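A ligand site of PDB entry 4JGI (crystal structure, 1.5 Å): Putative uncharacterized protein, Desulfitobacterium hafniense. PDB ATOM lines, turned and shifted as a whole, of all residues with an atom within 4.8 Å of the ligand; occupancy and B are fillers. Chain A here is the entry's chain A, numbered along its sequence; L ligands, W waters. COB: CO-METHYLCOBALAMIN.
O of Gly 179 sits close to O7R of the ligand.
OD1 of Asp 103 sits at hydrogen-bond distance from N52 of the ligand (2.8 Å).
N of Gly 179 is in hydrogen-bond range of O7R of the ligand (3.1 Å).
A nitrogen (N3B) of the ligand lies within hydrogen-bond range of the side-chain hydroxyl (OG) of Ser 147 (2.8 Å).
The backbone NH (N) of Val 180 lies within hydrogen-bond range of an oxygen (O4) of the ligand.
A ring nitrogen (NE2) of His 102 is bound to a cobalt atom (CO) of the ligand.
N of Ala 199 sits at hydrogen-bond distance from O8R of the ligand, at 3.1 Å.
An oxygen (O51) of the ligand is in hydrogen-bond range of the backbone NH of Asp 103, 2.9 Å away.
The side-chain carboxylate (OD1) of Asp 100 lies close to a nitrogen (N45) of the ligand.
The backbone NH (N) of Ile 104 is in hydrogen-bond range of an oxygen (O51) of the ligand, at 3.2 Å.
OD2 of Asp 100 is in hydrogen-bond range of N of Leu 150 (2.9 Å).
The side-chain amide nitrogen of Asn 198 sits at hydrogen-bond distance from the side-chain hydroxyl of Thr 197, at 3.4 Å.
OD1 of Asp 100 lies within hydrogen-bond range of ND1 of His 102 (2.8 Å).
OD2 of Asp 100 is in hydrogen-bond range of N of Val 149 (2.8 Å).
The backbone carbonyl oxygen of Ile 176 sits at hydrogen-bond distance from the backbone NH of Leu 146 (3.0 Å).
The backbone NH (N) of Gly 178 is in hydrogen-bond range of the backbone carbonyl oxygen (O) of Leu 146 (2.9 Å).
The backbone NH of Ser 196 sits at hydrogen-bond distance from the backbone carbonyl oxygen of Ile 177 (3.0 Å).
Water W2 lies within hydrogen-bond range of O34 of the ligand (2.6 Å) and N of Thr 151 (2.9 Å).
Water W16 lies within hydrogen-bond range of an oxygen (O5) of the ligand (2.7 Å), the backbone NH (N) of Gly 105 (2.9 Å) and the backbone NH (N) of Ile 104 (3.4 Å).
Water W14 lies within hydrogen-bond range of O5 of the ligand (2.8 Å) and N of Val 180 (2.9 Å).
Water W4 lies within hydrogen-bond range of O of Val 149 (2.7 Å), N33 of the ligand (3.1 Å) and OG1 of Thr 151 (3.2 Å).
The backbone carbonyl oxygen (O) of Gly 99 lies close to an oxygen (O44) of the ligand (3.0 Å).
The backbone NH (N) of Leu 101 lies close to a nitrogen (N45) of the ligand (2.9 Å).
Ile 60 touches the ligand.
Leu 63 touches the ligand.
CD1 of Leu 94 touches C5M of the ligand (3.9 Å).
CA of Gly 105 touches O2 of the ligand (3.3 Å).
Lys 106 touches the ligand (N to N3B, 3.7 Å).
CD1 of Ile 108 touches C3P of the ligand, 3.9 Å away.
CD1 of Phe 109 touches C6M of the ligand, 3.6 Å away.
Gly 145 touches the ligand (CA to C5M, 3.6 Å).
N of Leu 146 touches C5M of the ligand (3.7 Å).
Val 149 touches the ligand (CG2 to N33, 3.8 Å).
CD2 of Leu 150 touches O34 of the ligand (3.4 Å).
Ile 176 touches the ligand (O to C5M, 3.8 Å).
Gly 178 touches the ligand (CA to C9B, 3.6 Å).
OG of Ser 196 touches C7B of the ligand, at 3.0 Å.
CA of Asn 198 touches O8R of the ligand (3.4 Å).
Hydrophobic or aromatic side chains that line the ligand: Ile 60, Leu 63, Leu 94, Leu 101, His 102, Ile 104, Ile 108, Phe 109, Val 149, Leu 150, Ile 176, Val 180 and Ala 199.
Along chain A the residues within 4 Å of the ligand span positions 60 to 199.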
ATOM      1  N   ILE A  60     -19.321  12.928  12.080  1.00  0.00           N
ATOM      2  CA  ILE A  60     -20.765  12.745  11.855  1.00  0.00           C
ATOM      3  C   ILE A  60     -21.227  11.364  12.321  1.00  0.00           C
ATOM      4  O   ILE A  60     -22.293  11.226  12.912  1.00  0.00           O
ATOM      5  CB  ILE A  60     -21.082  12.938  10.329  1.00  0.00           C
ATOM      6  CG1 ILE A  60     -20.831  14.418  10.049  1.00  0.00           C
ATOM      7  CG2 ILE A  60     -22.499  12.542   9.919  1.00  0.00           C
ATOM      8  CD1 ILE A  60     -21.585  15.413  10.899  1.00  0.00           C
ATOM      9  N   LEU A  63     -22.221  11.204  15.838  1.00  0.00           N
ATOM     10  CA  LEU A  63     -23.497  11.789  16.140  1.00  0.00           C
ATOM     11  C   LEU A  63     -24.678  10.839  15.790  1.00  0.00           C
ATOM     12  O   LEU A  63     -25.695  10.847  16.484  1.00  0.00           O
ATOM     13  CB  LEU A  63     -23.707  13.116  15.476  1.00  0.00           C
ATOM     14  CG  LEU A  63     -22.701  14.178  15.780  1.00  0.00           C
ATOM     15  CD1 LEU A  63     -23.045  15.427  14.957  1.00  0.00           C
ATOM     16  CD2 LEU A  63     -22.644  14.567  17.223  1.00  0.00           C
ATOM     17  N   LEU A  94     -40.797  19.905  12.895  1.00  0.00           N
ATOM     18  CA  LEU A  94     -39.456  19.859  12.279  1.00  0.00           C
ATOM     19  C   LEU A  94     -39.564  19.741  10.778  1.00  0.00           C
ATOM     20  O   LEU A  94     -40.337  18.924  10.317  1.00  0.00           O
ATOM     21  CB  LEU A  94     -38.693  18.662  12.867  1.00  0.00           C
ATOM     22  CG  LEU A  94     -37.271  18.382  12.392  1.00  0.00           C
ATOM     23  CD1 LEU A  94     -36.353  19.581  12.720  1.00  0.00           C
ATOM     24  CD2 LEU A  94     -36.707  17.101  13.027  1.00  0.00           C
ATOM     25  N   GLY A  99     -37.262  24.610  -0.889  1.00  0.00           N
ATOM     26  CA  GLY A  99     -36.085  24.920  -1.695  1.00  0.00           C
ATOM     27  C   GLY A  99     -34.970  23.969  -1.408  1.00  0.00           C
ATOM     28  O   GLY A  99     -34.004  23.956  -2.165  1.00  0.00           O
ATOM     29  N   ASP A 100     -35.131  23.160  -0.332  1.00  0.00           N
ATOM     30  CA  ASP A 100     -34.075  22.296   0.130  1.00  0.00           C
ATOM     31  C   ASP A 100     -34.429  20.825   0.237  1.00  0.00           C
ATOM     32  O   ASP A 100     -35.468  20.434   0.689  1.00  0.00           O
ATOM     33  CB  ASP A 100     -33.551  22.829   1.453  1.00  0.00           C
ATOM     34  CG  ASP A 100     -32.057  22.713   1.589  1.00  0.00           C
ATOM     35  OD1 ASP A 100     -31.618  21.534   1.748  1.00  0.00           O
ATOM     36  OD2 ASP A 100     -31.309  23.726   1.536  1.00  0.00           O
ATOM     37  N   LEU A 101     -33.462  19.972  -0.196  1.00  0.00           N
ATOM     38  CA  LEU A 101     -33.667  18.515  -0.136  1.00  0.00           C
ATOM     39  C   LEU A 101     -32.706  17.831   0.859  1.00  0.00           C
ATOM     40  O   LEU A 101     -32.688  16.539   0.939  1.00  0.00           O
ATOM     41  CB  LEU A 101     -33.442  17.872  -1.500  1.00  0.00           C
ATOM     42  CG  LEU A 101     -34.373  18.449  -2.555  1.00  0.00           C
ATOM     43  CD1 LEU A 101     -34.056  17.806  -3.874  1.00  0.00           C
ATOM     44  CD2 LEU A 101     -35.832  18.233  -2.289  1.00  0.00           C
ATOM     45  N   HIS A 102     -31.938  18.586   1.590  1.00  0.00           N
ATOM     46  CA  HIS A 102     -30.967  18.001   2.524  1.00  0.00           C
ATOM     47  C   HIS A 102     -31.625  17.598   3.816  1.00  0.00           C
ATOM     48  O   HIS A 102     -32.228  18.518   4.413  1.00  0.00           O
ATOM     49  CB  HIS A 102     -29.788  18.964   2.743  1.00  0.00           C
ATOM     50  CG  HIS A 102     -28.992  19.265   1.494  1.00  0.00           C
ATOM     51  ND1 HIS A 102     -29.327  20.305   0.663  1.00  0.00           N
ATOM     52  CD2 HIS A 102     -27.787  18.823   1.049  1.00  0.00           C
ATOM     53  CE1 HIS A 102     -28.449  20.391  -0.321  1.00  0.00           C
ATOM     54  NE2 HIS A 102     -27.521  19.480  -0.117  1.00  0.00           N
ATOM     55  N   ASP A 103     -31.613  16.330   4.217  1.00  0.00           N
ATOM     56  CA  ASP A 103     -32.193  15.866   5.456  1.00  0.00           C
ATOM     57  C   ASP A 103     -31.341  14.980   6.313  1.00  0.00           C
ATOM     58  O   ASP A 103     -31.752  14.619   7.410  1.00  0.00           O
ATOM     59  CB  ASP A 103     -33.522  15.176   5.228  1.00  0.00           C
ATOM     60  CG  ASP A 103     -33.438  13.876   4.556  1.00  0.00           C
ATOM     61  OD1 ASP A 103     -32.303  13.434   4.217  1.00  0.00           O
ATOM     62  OD2 ASP A 103     -34.555  13.223   4.334  1.00  0.00           O
ATOM     63  N   ILE A 104     -30.091  14.704   5.911  1.00  0.00           N
ATOM     64  CA  ILE A 104     -29.301  13.854   6.804  1.00  0.00           C
ATOM     65  C   ILE A 104     -29.138  14.439   8.190  1.00  0.00           C
ATOM     66  O   ILE A 104     -29.265  13.764   9.236  1.00  0.00           O
ATOM     67  CB  ILE A 104     -27.950  13.528   6.162  1.00  0.00           C
ATOM     68  CG1 ILE A 104     -28.141  12.716   4.916  1.00  0.00           C
ATOM     69  CG2 ILE A 104     -26.960  12.877   7.145  1.00  0.00           C
ATOM     70  CD1 ILE A 104     -26.942  12.610   3.982  1.00  0.00           C
ATOM     71  N   GLY A 105     -28.795  15.721   8.216  1.00  0.00           N
ATOM     72  CA  GLY A 105     -28.637  16.422   9.485  1.00  0.00           C
ATOM     73  C   GLY A 105     -29.891  16.582  10.324  1.00  0.00           C
ATOM     74  O   GLY A 105     -29.933  16.349  11.553  1.00  0.00           O
ATOM     75  N   LYS A 106     -30.938  16.968   9.635  1.00  0.00           N
ATOM     76  CA  LYS A 106     -32.260  17.098  10.289  1.00  0.00           C
ATOM     77  C   LYS A 106     -32.584  15.784  10.921  1.00  0.00           C
ATOM     78  O   LYS A 106     -33.134  15.753  12.015  1.00  0.00           O
ATOM     79  CB  LYS A 106     -33.293  17.466   9.206  1.00  0.00           C
ATOM     80  CG  LYS A 106     -34.727  17.473   9.751  1.00  0.00           C
ATOM     81  CD  LYS A 106     -35.761  17.808   8.726  1.00  0.00           C
ATOM     82  CE  LYS A 106     -35.980  16.713   7.634  1.00  0.00           C
ATOM     83  NZ  LYS A 106     -36.631  15.438   7.944  1.00  0.00           N
ATOM     84  N   ILE A 108     -30.564  13.353  12.021  1.00  0.00           N
ATOM     85  CA  ILE A 108     -29.724  13.181  13.205  1.00  0.00           C
ATOM     86  C   ILE A 108     -30.340  13.890  14.394  1.00  0.00           C
ATOM     87  O   ILE A 108     -30.524  13.322  15.454  1.00  0.00           O
ATOM     88  CB  ILE A 108     -28.257  13.614  12.934  1.00  0.00           C
ATOM     89  CG1 ILE A 108     -27.644  12.728  11.888  1.00  0.00           C
ATOM     90  CG2 ILE A 108     -27.482  13.629  14.206  1.00  0.00           C
ATOM     91  CD1 ILE A 108     -26.254  13.157  11.446  1.00  0.00           C
ATOM     92  N   PHE A 109     -30.761  15.125  14.198  1.00  0.00           N
ATOM     93  CA  PHE A 109     -31.460  15.849  15.220  1.00  0.00           C
ATOM     94  C   PHE A 109     -32.772  15.209  15.610  1.00  0.00           C
ATOM     95  O   PHE A 109     -33.032  15.093  16.802  1.00  0.00           O
ATOM     96  CB  PHE A 109     -31.627  17.298  14.778  1.00  0.00           C
ATOM     97  CG  PHE A 109     -32.460  18.106  15.743  1.00  0.00           C
ATOM     98  CD1 PHE A 109     -31.925  18.542  16.969  1.00  0.00           C
ATOM     99  CD2 PHE A 109     -33.763  18.391  15.489  1.00  0.00           C
ATOM    100  CE1 PHE A 109     -32.725  19.217  17.911  1.00  0.00           C
ATOM    101  CE2 PHE A 109     -34.530  19.082  16.396  1.00  0.00           C
ATOM    102  CZ  PHE A 109     -34.009  19.517  17.604  1.00  0.00           C
ATOM    103  N   GLY A 145     -38.442  23.659  14.466  1.00  0.00           N
ATOM    104  CA  GLY A 145     -37.061  23.477  14.021  1.00  0.00           C
ATOM    105  C   GLY A 145     -37.029  23.409  12.499  1.00  0.00           C
ATOM    106  O   GLY A 145     -37.799  22.643  11.880  1.00  0.00           O
ATOM    107  N   LEU A 146     -36.182  24.231  11.922  1.00  0.00           N
ATOM    108  CA  LEU A 146     -36.079  24.432  10.513  1.00  0.00           C
ATOM    109  C   LEU A 146     -34.639  24.135  10.043  1.00  0.00           C
ATOM    110  O   LEU A 146     -33.671  24.654  10.614  1.00  0.00           O
ATOM    111  CB  LEU A 146     -36.404  25.841  10.065  1.00  0.00           C
ATOM    112  CG  LEU A 146     -37.775  26.365  10.531  1.00  0.00           C
ATOM    113  CD1 LEU A 146     -37.949  27.845  10.196  1.00  0.00           C
ATOM    114  CD2 LEU A 146     -38.903  25.568  10.026  1.00  0.00           C
ATOM    115  N   SER A 147     -34.530  23.293   9.024  1.00  0.00           N
ATOM    116  CA  SER A 147     -33.258  22.912   8.369  1.00  0.00           C
ATOM    117  C   SER A 147     -33.156  23.477   6.955  1.00  0.00           C
ATOM    118  O   SER A 147     -34.113  23.440   6.227  1.00  0.00           O
ATOM    119  CB  SER A 147     -33.125  21.352   8.373  1.00  0.00           C
ATOM    120  OG  SER A 147     -31.811  20.901   7.988  1.00  0.00           O
ATOM    121  N   VAL A 149     -29.891  24.630   3.743  1.00  0.00           N
ATOM    122  CA  VAL A 149     -28.550  25.043   3.360  1.00  0.00           C
ATOM    123  C   VAL A 149     -28.532  26.037   2.191  1.00  0.00           C
ATOM    124  O   VAL A 149     -27.797  27.044   2.262  1.00  0.00           O
ATOM    125  CB  VAL A 149     -27.593  23.843   3.050  1.00  0.00           C
ATOM    126  CG1 VAL A 149     -28.317  22.856   2.210  1.00  0.00           C
ATOM    127  CG2 VAL A 149     -26.342  24.328   2.293  1.00  0.00           C
ATOM    128  N   LEU A 150     -29.289  25.799   1.174  1.00  0.00           N
ATOM    129  CA  LEU A 150     -29.253  26.720   0.023  1.00  0.00           C
ATOM    130  C   LEU A 150     -29.749  28.114   0.445  1.00  0.00           C
ATOM    131  O   LEU A 150     -30.559  28.257   1.353  1.00  0.00           O
ATOM    132  CB  LEU A 150     -30.170  26.216  -1.048  1.00  0.00           C
ATOM    133  CG  LEU A 150     -29.855  24.815  -1.632  1.00  0.00           C
ATOM    134  CD1 LEU A 150     -30.658  24.553  -2.889  1.00  0.00           C
ATOM    135  CD2 LEU A 150     -28.384  24.628  -1.839  1.00  0.00           C
ATOM    136  N   THR A 151     -29.318  29.117  -0.278  1.00  0.00           N
ATOM    137  CA  THR A 151     -29.705  30.506   0.073  1.00  0.00           C
ATOM    138  C   THR A 151     -31.203  30.670  -0.047  1.00  0.00           C
ATOM    139  O   THR A 151     -31.800  31.310   0.801  1.00  0.00           O
ATOM    140  CB  THR A 151     -28.896  31.553  -0.746  1.00  0.00           C
ATOM    141  OG1 THR A 151     -27.499  31.371  -0.477  1.00  0.00           O
ATOM    142  CG2 THR A 151     -29.266  32.948  -0.337  1.00  0.00           C
ATOM    143  N   ILE A 176     -35.818  27.239  16.293  1.00  0.00           N
ATOM    144  CA  ILE A 176     -34.398  26.876  16.197  1.00  0.00           C
ATOM    145  C   ILE A 176     -34.116  26.515  14.735  1.00  0.00           C
ATOM    146  O   ILE A 176     -34.898  25.812  14.106  1.00  0.00           O
ATOM    147  CB  ILE A 176     -33.999  25.783  17.194  1.00  0.00           C
ATOM    148  CG1 ILE A 176     -32.489  25.547  17.148  1.00  0.00           C
ATOM    149  CG2 ILE A 176     -34.726  24.470  16.949  1.00  0.00           C
ATOM    150  CD1 ILE A 176     -32.004  24.661  18.278  1.00  0.00           C
ATOM    151  N   ILE A 177     -32.974  26.984  14.222  1.00  0.00           N
ATOM    152  CA  ILE A 177     -32.552  26.669  12.873  1.00  0.00           C
ATOM    153  C   ILE A 177     -31.238  25.880  12.928  1.00  0.00           C
ATOM    154  O   ILE A 177     -30.417  26.010  13.836  1.00  0.00           O
ATOM    155  CB  ILE A 177     -32.433  27.904  11.961  1.00  0.00           C
ATOM    156  CG1 ILE A 177     -31.293  28.829  12.490  1.00  0.00           C
ATOM    157  CG2 ILE A 177     -33.815  28.592  11.927  1.00  0.00           C
ATOM    158  CD1 ILE A 177     -31.005  29.980  11.577  1.00  0.00           C
ATOM    159  N   GLY A 178     -31.081  25.071  11.874  1.00  0.00           N
ATOM    160  CA  GLY A 178     -29.867  24.308  11.673  1.00  0.00           C
ATOM    161  C   GLY A 178     -29.637  24.068  10.216  1.00  0.00           C
ATOM    162  O   GLY A 178     -30.459  24.355   9.361  1.00  0.00           O
ATOM    163  N   GLY A 179     -28.445  23.572   9.921  1.00  0.00           N
ATOM    164  CA  GLY A 179     -28.044  23.300   8.530  1.00  0.00           C
ATOM    165  C   GLY A 179     -26.611  23.749   8.288  1.00  0.00           C
ATOM    166  O   GLY A 179     -25.998  24.485   9.076  1.00  0.00           O
ATOM    167  N   VAL A 180     -26.053  23.296   7.173  1.00  0.00           N
ATOM    168  CA  VAL A 180     -24.658  23.584   6.867  1.00  0.00           C
ATOM    169  C   VAL A 180     -24.128  25.010   7.132  1.00  0.00           C
ATOM    170  O   VAL A 180     -23.159  25.178   7.813  1.00  0.00           O
ATOM    171  CB  VAL A 180     -24.293  23.102   5.456  1.00  0.00           C
ATOM    172  CG1 VAL A 180     -22.922  23.642   5.073  1.00  0.00           C
ATOM    173  CG2 VAL A 180     -24.301  21.559   5.407  1.00  0.00           C
ATOM    174  N   SER A 196     -28.222  25.988  15.894  1.00  0.00           N
ATOM    175  CA  SER A 196     -27.388  24.898  16.492  1.00  0.00           C
ATOM    176  C   SER A 196     -26.016  24.828  15.889  1.00  0.00           C
ATOM    177  O   SER A 196     -25.913  24.896  14.678  1.00  0.00           O
ATOM    178  CB  SER A 196     -28.082  23.516  16.386  1.00  0.00           C
ATOM    179  OG  SER A 196     -28.731  23.437  15.165  1.00  0.00           O
ATOM    180  N   THR A 197     -25.015  24.431  16.676  1.00  0.00           N
ATOM    181  CA  THR A 197     -23.692  24.095  16.038  1.00  0.00           C
ATOM    182  C   THR A 197     -23.646  22.637  15.456  1.00  0.00           C
ATOM    183  O   THR A 197     -22.988  22.287  14.479  1.00  0.00           O
ATOM    184  CB  THR A 197     -22.557  24.287  17.049  1.00  0.00           C
ATOM    185  OG1 THR A 197     -22.787  23.462  18.198  1.00  0.00           O
ATOM    186  CG2 THR A 197     -22.480  25.791  17.481  1.00  0.00           C
ATOM    187  N   ASN A 198     -24.430  21.805  16.082  1.00  0.00           N
ATOM    188  CA  ASN A 198     -24.497  20.451  15.780  1.00  0.00           C
ATOM    189  C   ASN A 198     -25.758  19.964  16.467  1.00  0.00           C
ATOM    190  O   ASN A 198     -26.337  20.667  17.299  1.00  0.00           O
ATOM    191  CB  ASN A 198     -23.280  19.636  16.147  1.00  0.00           C
ATOM    192  CG  ASN A 198     -23.073  19.555  17.625  1.00  0.00           C
ATOM    193  OD1 ASN A 198     -23.881  18.970  18.318  1.00  0.00           O
ATOM    194  ND2 ASN A 198     -21.961  20.155  18.129  1.00  0.00           N
ATOM    195  N   ALA A 199     -26.217  18.807  16.089  1.00  0.00           N
ATOM    196  CA  ALA A 199     -27.476  18.336  16.521  1.00  0.00           C
ATOM    197  C   ALA A 199     -27.576  18.138  18.032  1.00  0.00           C
ATOM    198  O   ALA A 199     -28.635  18.344  18.625  1.00  0.00           O
ATOM    199  CB  ALA A 199     -27.823  17.039  15.828  1.00  0.00           C
ATOM    200  N   GLY A 202     -28.116  21.383  19.506  1.00  0.00           N
ATOM    201  CA  GLY A 202     -29.501  21.778  19.323  1.00  0.00           C
ATOM    202  C   GLY A 202     -30.423  21.167  20.351  1.00  0.00           C
ATOM    203  O   GLY A 202     -31.373  21.820  20.857  1.00  0.00           O
HETATM  204 CO   COB L   1     -25.680  18.945  -1.811  1.00  0.00          CO
HETATM  205  N21 COB L   1     -24.718  20.522  -1.597  1.00  0.00           N
HETATM  206  N22 COB L   1     -26.652  19.714  -3.275  1.00  0.00           N
HETATM  207  N23 COB L   1     -26.615  17.286  -1.825  1.00  0.00           N
HETATM  208  N24 COB L   1     -24.443  18.312  -0.553  1.00  0.00           N
HETATM  209  C1  COB L   1     -23.877  20.697  -0.440  1.00  0.00           C
HETATM  210  C20 COB L   1     -24.737  21.014   0.765  1.00  0.00           C
HETATM  211  C2  COB L   1     -22.850  21.826  -0.797  1.00  0.00           C
HETATM  212  C25 COB L   1     -22.320  22.653   0.387  1.00  0.00           C
HETATM  213  C26 COB L   1     -21.644  21.206  -1.603  1.00  0.00           C
HETATM  214  C27 COB L   1     -20.550  22.320  -2.057  1.00  0.00           C
HETATM  215  O28 COB L   1     -19.468  22.456  -1.411  1.00  0.00           O
HETATM  216  N29 COB L   1     -20.856  23.037  -3.108  1.00  0.00           N
HETATM  217  C3  COB L   1     -23.667  22.623  -1.856  1.00  0.00           C
HETATM  218  C30 COB L   1     -24.496  23.799  -1.307  1.00  0.00           C
HETATM  219  C31 COB L   1     -23.811  25.145  -1.429  1.00  0.00           C
HETATM  220  C32 COB L   1     -24.726  26.299  -1.082  1.00  0.00           C
HETATM  221  O34 COB L   1     -25.602  26.650  -1.858  1.00  0.00           O
HETATM  222  N33 COB L   1     -24.519  26.878   0.070  1.00  0.00           N
HETATM  223  C4  COB L   1     -24.614  21.596  -2.413  1.00  0.00           C
HETATM  224  C5  COB L   1     -25.321  21.713  -3.702  1.00  0.00           C
HETATM  225  C35 COB L   1     -24.864  22.797  -4.645  1.00  0.00           C
HETATM  226  C6  COB L   1     -26.326  20.849  -4.033  1.00  0.00           C
HETATM  227  C7  COB L   1     -27.228  20.832  -5.230  1.00  0.00           C
HETATM  228  C36 COB L   1     -27.661  22.225  -5.721  1.00  0.00           C
HETATM  229  C37 COB L   1     -26.433  20.143  -6.388  1.00  0.00           C
HETATM  230  C38 COB L   1     -27.235  20.079  -7.671  1.00  0.00           C
HETATM  231  O39 COB L   1     -28.216  19.381  -7.873  1.00  0.00           O
HETATM  232  N40 COB L   1     -26.752  20.888  -8.582  1.00  0.00           N
HETATM  233  C8  COB L   1     -28.434  19.995  -4.802  1.00  0.00           C
HETATM  234  C41 COB L   1     -29.481  20.862  -4.067  1.00  0.00           C
HETATM  235  C42 COB L   1     -30.695  20.123  -3.605  1.00  0.00           C
HETATM  236  C43 COB L   1     -31.638  21.058  -2.880  1.00  0.00           C
HETATM  237  O44 COB L   1     -32.564  21.649  -3.483  1.00  0.00           O
HETATM  238  N45 COB L   1     -31.358  21.288  -1.622  1.00  0.00           N
HETATM  239  C9  COB L   1     -27.731  19.107  -3.795  1.00  0.00           C
HETATM  240  C10 COB L   1     -28.276  17.859  -3.502  1.00  0.00           C
HETATM  241  C11 COB L   1     -27.656  16.942  -2.545  1.00  0.00           C
HETATM  242  C12 COB L   1     -28.217  15.562  -2.317  1.00  0.00           C
HETATM  243  C46 COB L   1     -27.552  14.667  -3.395  1.00  0.00           C
HETATM  244  C47 COB L   1     -29.749  15.393  -2.370  1.00  0.00           C
HETATM  245  C13 COB L   1     -27.446  15.168  -1.034  1.00  0.00           C
HETATM  246  C48 COB L   1     -28.313  15.288   0.240  1.00  0.00           C
HETATM  247  C49 COB L   1     -28.986  13.975   0.600  1.00  0.00           C
HETATM  248  C50 COB L   1     -29.887  14.019   1.819  1.00  0.00           C
HETATM  249  O51 COB L   1     -29.663  14.818   2.739  1.00  0.00           O
HETATM  250  N52 COB L   1     -30.858  13.118   1.856  1.00  0.00           N
HETATM  251  C14 COB L   1     -26.314  16.187  -0.851  1.00  0.00           C
HETATM  252  C15 COB L   1     -25.262  16.133   0.012  1.00  0.00           C
HETATM  253  C53 COB L   1     -25.142  14.899   0.879  1.00  0.00           C
HETATM  254  C16 COB L   1     -24.320  17.192   0.164  1.00  0.00           C
HETATM  255  C17 COB L   1     -23.083  17.228   1.044  1.00  0.00           C
HETATM  256  C54 COB L   1     -22.044  16.332   0.337  1.00  0.00           C
HETATM  257  C55 COB L   1     -23.264  16.755   2.515  1.00  0.00           C
HETATM  258  C56 COB L   1     -24.392  17.448   3.295  1.00  0.00           C
HETATM  259  C57 COB L   1     -24.643  16.708   4.582  1.00  0.00           C
HETATM  260  O58 COB L   1     -25.511  15.826   4.643  1.00  0.00           O
HETATM  261  N59 COB L   1     -23.829  16.997   5.604  1.00  0.00           N
HETATM  262  C18 COB L   1     -22.713  18.719   1.030  1.00  0.00           C
HETATM  263  C60 COB L   1     -21.238  19.021   1.244  1.00  0.00           C
HETATM  264  C61 COB L   1     -20.805  18.893   2.684  1.00  0.00           C
HETATM  265  O63 COB L   1     -21.370  19.547   3.569  1.00  0.00           O
HETATM  266  N62 COB L   1     -19.758  18.135   2.905  1.00  0.00           N
HETATM  267  C19 COB L   1     -23.290  19.208  -0.307  1.00  0.00           C
HETATM  268  C1P COB L   1     -23.859  16.290   6.873  1.00  0.00           C
HETATM  269  C2P COB L   1     -24.958  16.789   7.829  1.00  0.00           C
HETATM  270  C3P COB L   1     -24.969  15.924   9.064  1.00  0.00           C
HETATM  271  O3  COB L   1     -24.533  18.122   8.184  1.00  0.00           O
HETATM  272  O4  COB L   1     -24.857  20.496   8.636  1.00  0.00           O
HETATM  273  O5  COB L   1     -26.632  19.251   7.284  1.00  0.00           O
HETATM  274  P   COB L   1     -25.624  19.297   8.393  1.00  0.00           P
HETATM  275  O2  COB L   1     -26.460  18.846   9.743  1.00  0.00           O
HETATM  276  C3R COB L   1     -25.892  19.034  11.044  1.00  0.00           C
HETATM  277  C2R COB L   1     -26.166  20.439  11.621  1.00  0.00           C
HETATM  278  O7R COB L   1     -26.330  21.492  10.677  1.00  0.00           O
HETATM  279  C1R COB L   1     -27.403  20.196  12.478  1.00  0.00           C
HETATM  280  O6R COB L   1     -27.299  18.873  12.937  1.00  0.00           O
HETATM  281  C4R COB L   1     -26.613  18.051  11.957  1.00  0.00           C
HETATM  282  C5R COB L   1     -25.668  17.137  12.721  1.00  0.00           C
HETATM  283  O8R COB L   1     -24.801  17.887  13.535  1.00  0.00           O
HETATM  284  N1B COB L   1     -28.709  20.361  11.830  1.00  0.00           N
HETATM  285  C8B COB L   1     -29.848  20.747  12.523  1.00  0.00           C
HETATM  286  C2B COB L   1     -29.084  20.259  10.524  1.00  0.00           C
HETATM  287  N3B COB L   1     -30.360  20.521  10.324  1.00  0.00           N
HETATM  288  C9B COB L   1     -30.852  20.842  11.574  1.00  0.00           C
HETATM  289  C4B COB L   1     -32.132  21.236  11.976  1.00  0.00           C
HETATM  290  C5B COB L   1     -32.348  21.624  13.295  1.00  0.00           C
HETATM  291  C5M COB L   1     -33.704  22.206  13.704  1.00  0.00           C
HETATM  292  C6B COB L   1     -31.305  21.532  14.237  1.00  0.00           C
HETATM  293  C6M COB L   1     -31.561  21.872  15.681  1.00  0.00           C
HETATM  294  C7B COB L   1     -30.064  21.039  13.840  1.00  0.00           C
HETATM  295  O   HOH W   1     -21.587  18.728   6.028  1.00  0.00           O
HETATM  296  O   HOH W   2     -27.140  28.712  -2.140  1.00  0.00           O
HETATM  297  O   HOH W   3     -22.185  20.548   8.215  1.00  0.00           O
HETATM  298  O   HOH W   4     -26.230  29.113   1.410  1.00  0.00           O
HETATM  299  O   HOH W   5     -18.626  21.439   0.927  1.00  0.00           O
HETATM  300  O   HOH W   6     -32.954  21.128  -6.459  1.00  0.00           O
HETATM  301  O   HOH W   7     -18.214  17.015   4.956  1.00  0.00           O
HETATM  302  O   HOH W   8     -31.321  11.698  -0.779  1.00  0.00           O
HETATM  303  O   HOH W   9     -28.495  16.685  -6.972  1.00  0.00           O
HETATM  304  O   HOH W  10     -22.075  26.252   1.564  1.00  0.00           O
HETATM  305  O   HOH W  11     -30.590  19.702  -8.875  1.00  0.00           O
HETATM  306  O   HOH W  12     -22.774  19.095  12.273  1.00  0.00           O
HETATM  307  O   HOH W  13     -28.057  21.302 -11.238  1.00  0.00           O
HETATM  308  O   HOH W  14     -27.800  21.338   5.910  1.00  0.00           O
HETATM  309  O   HOH W  15     -24.558  22.775  -8.559  1.00  0.00           O
HETATM  310  O   HOH W  16     -28.346  17.583   6.071  1.00  0.00           O
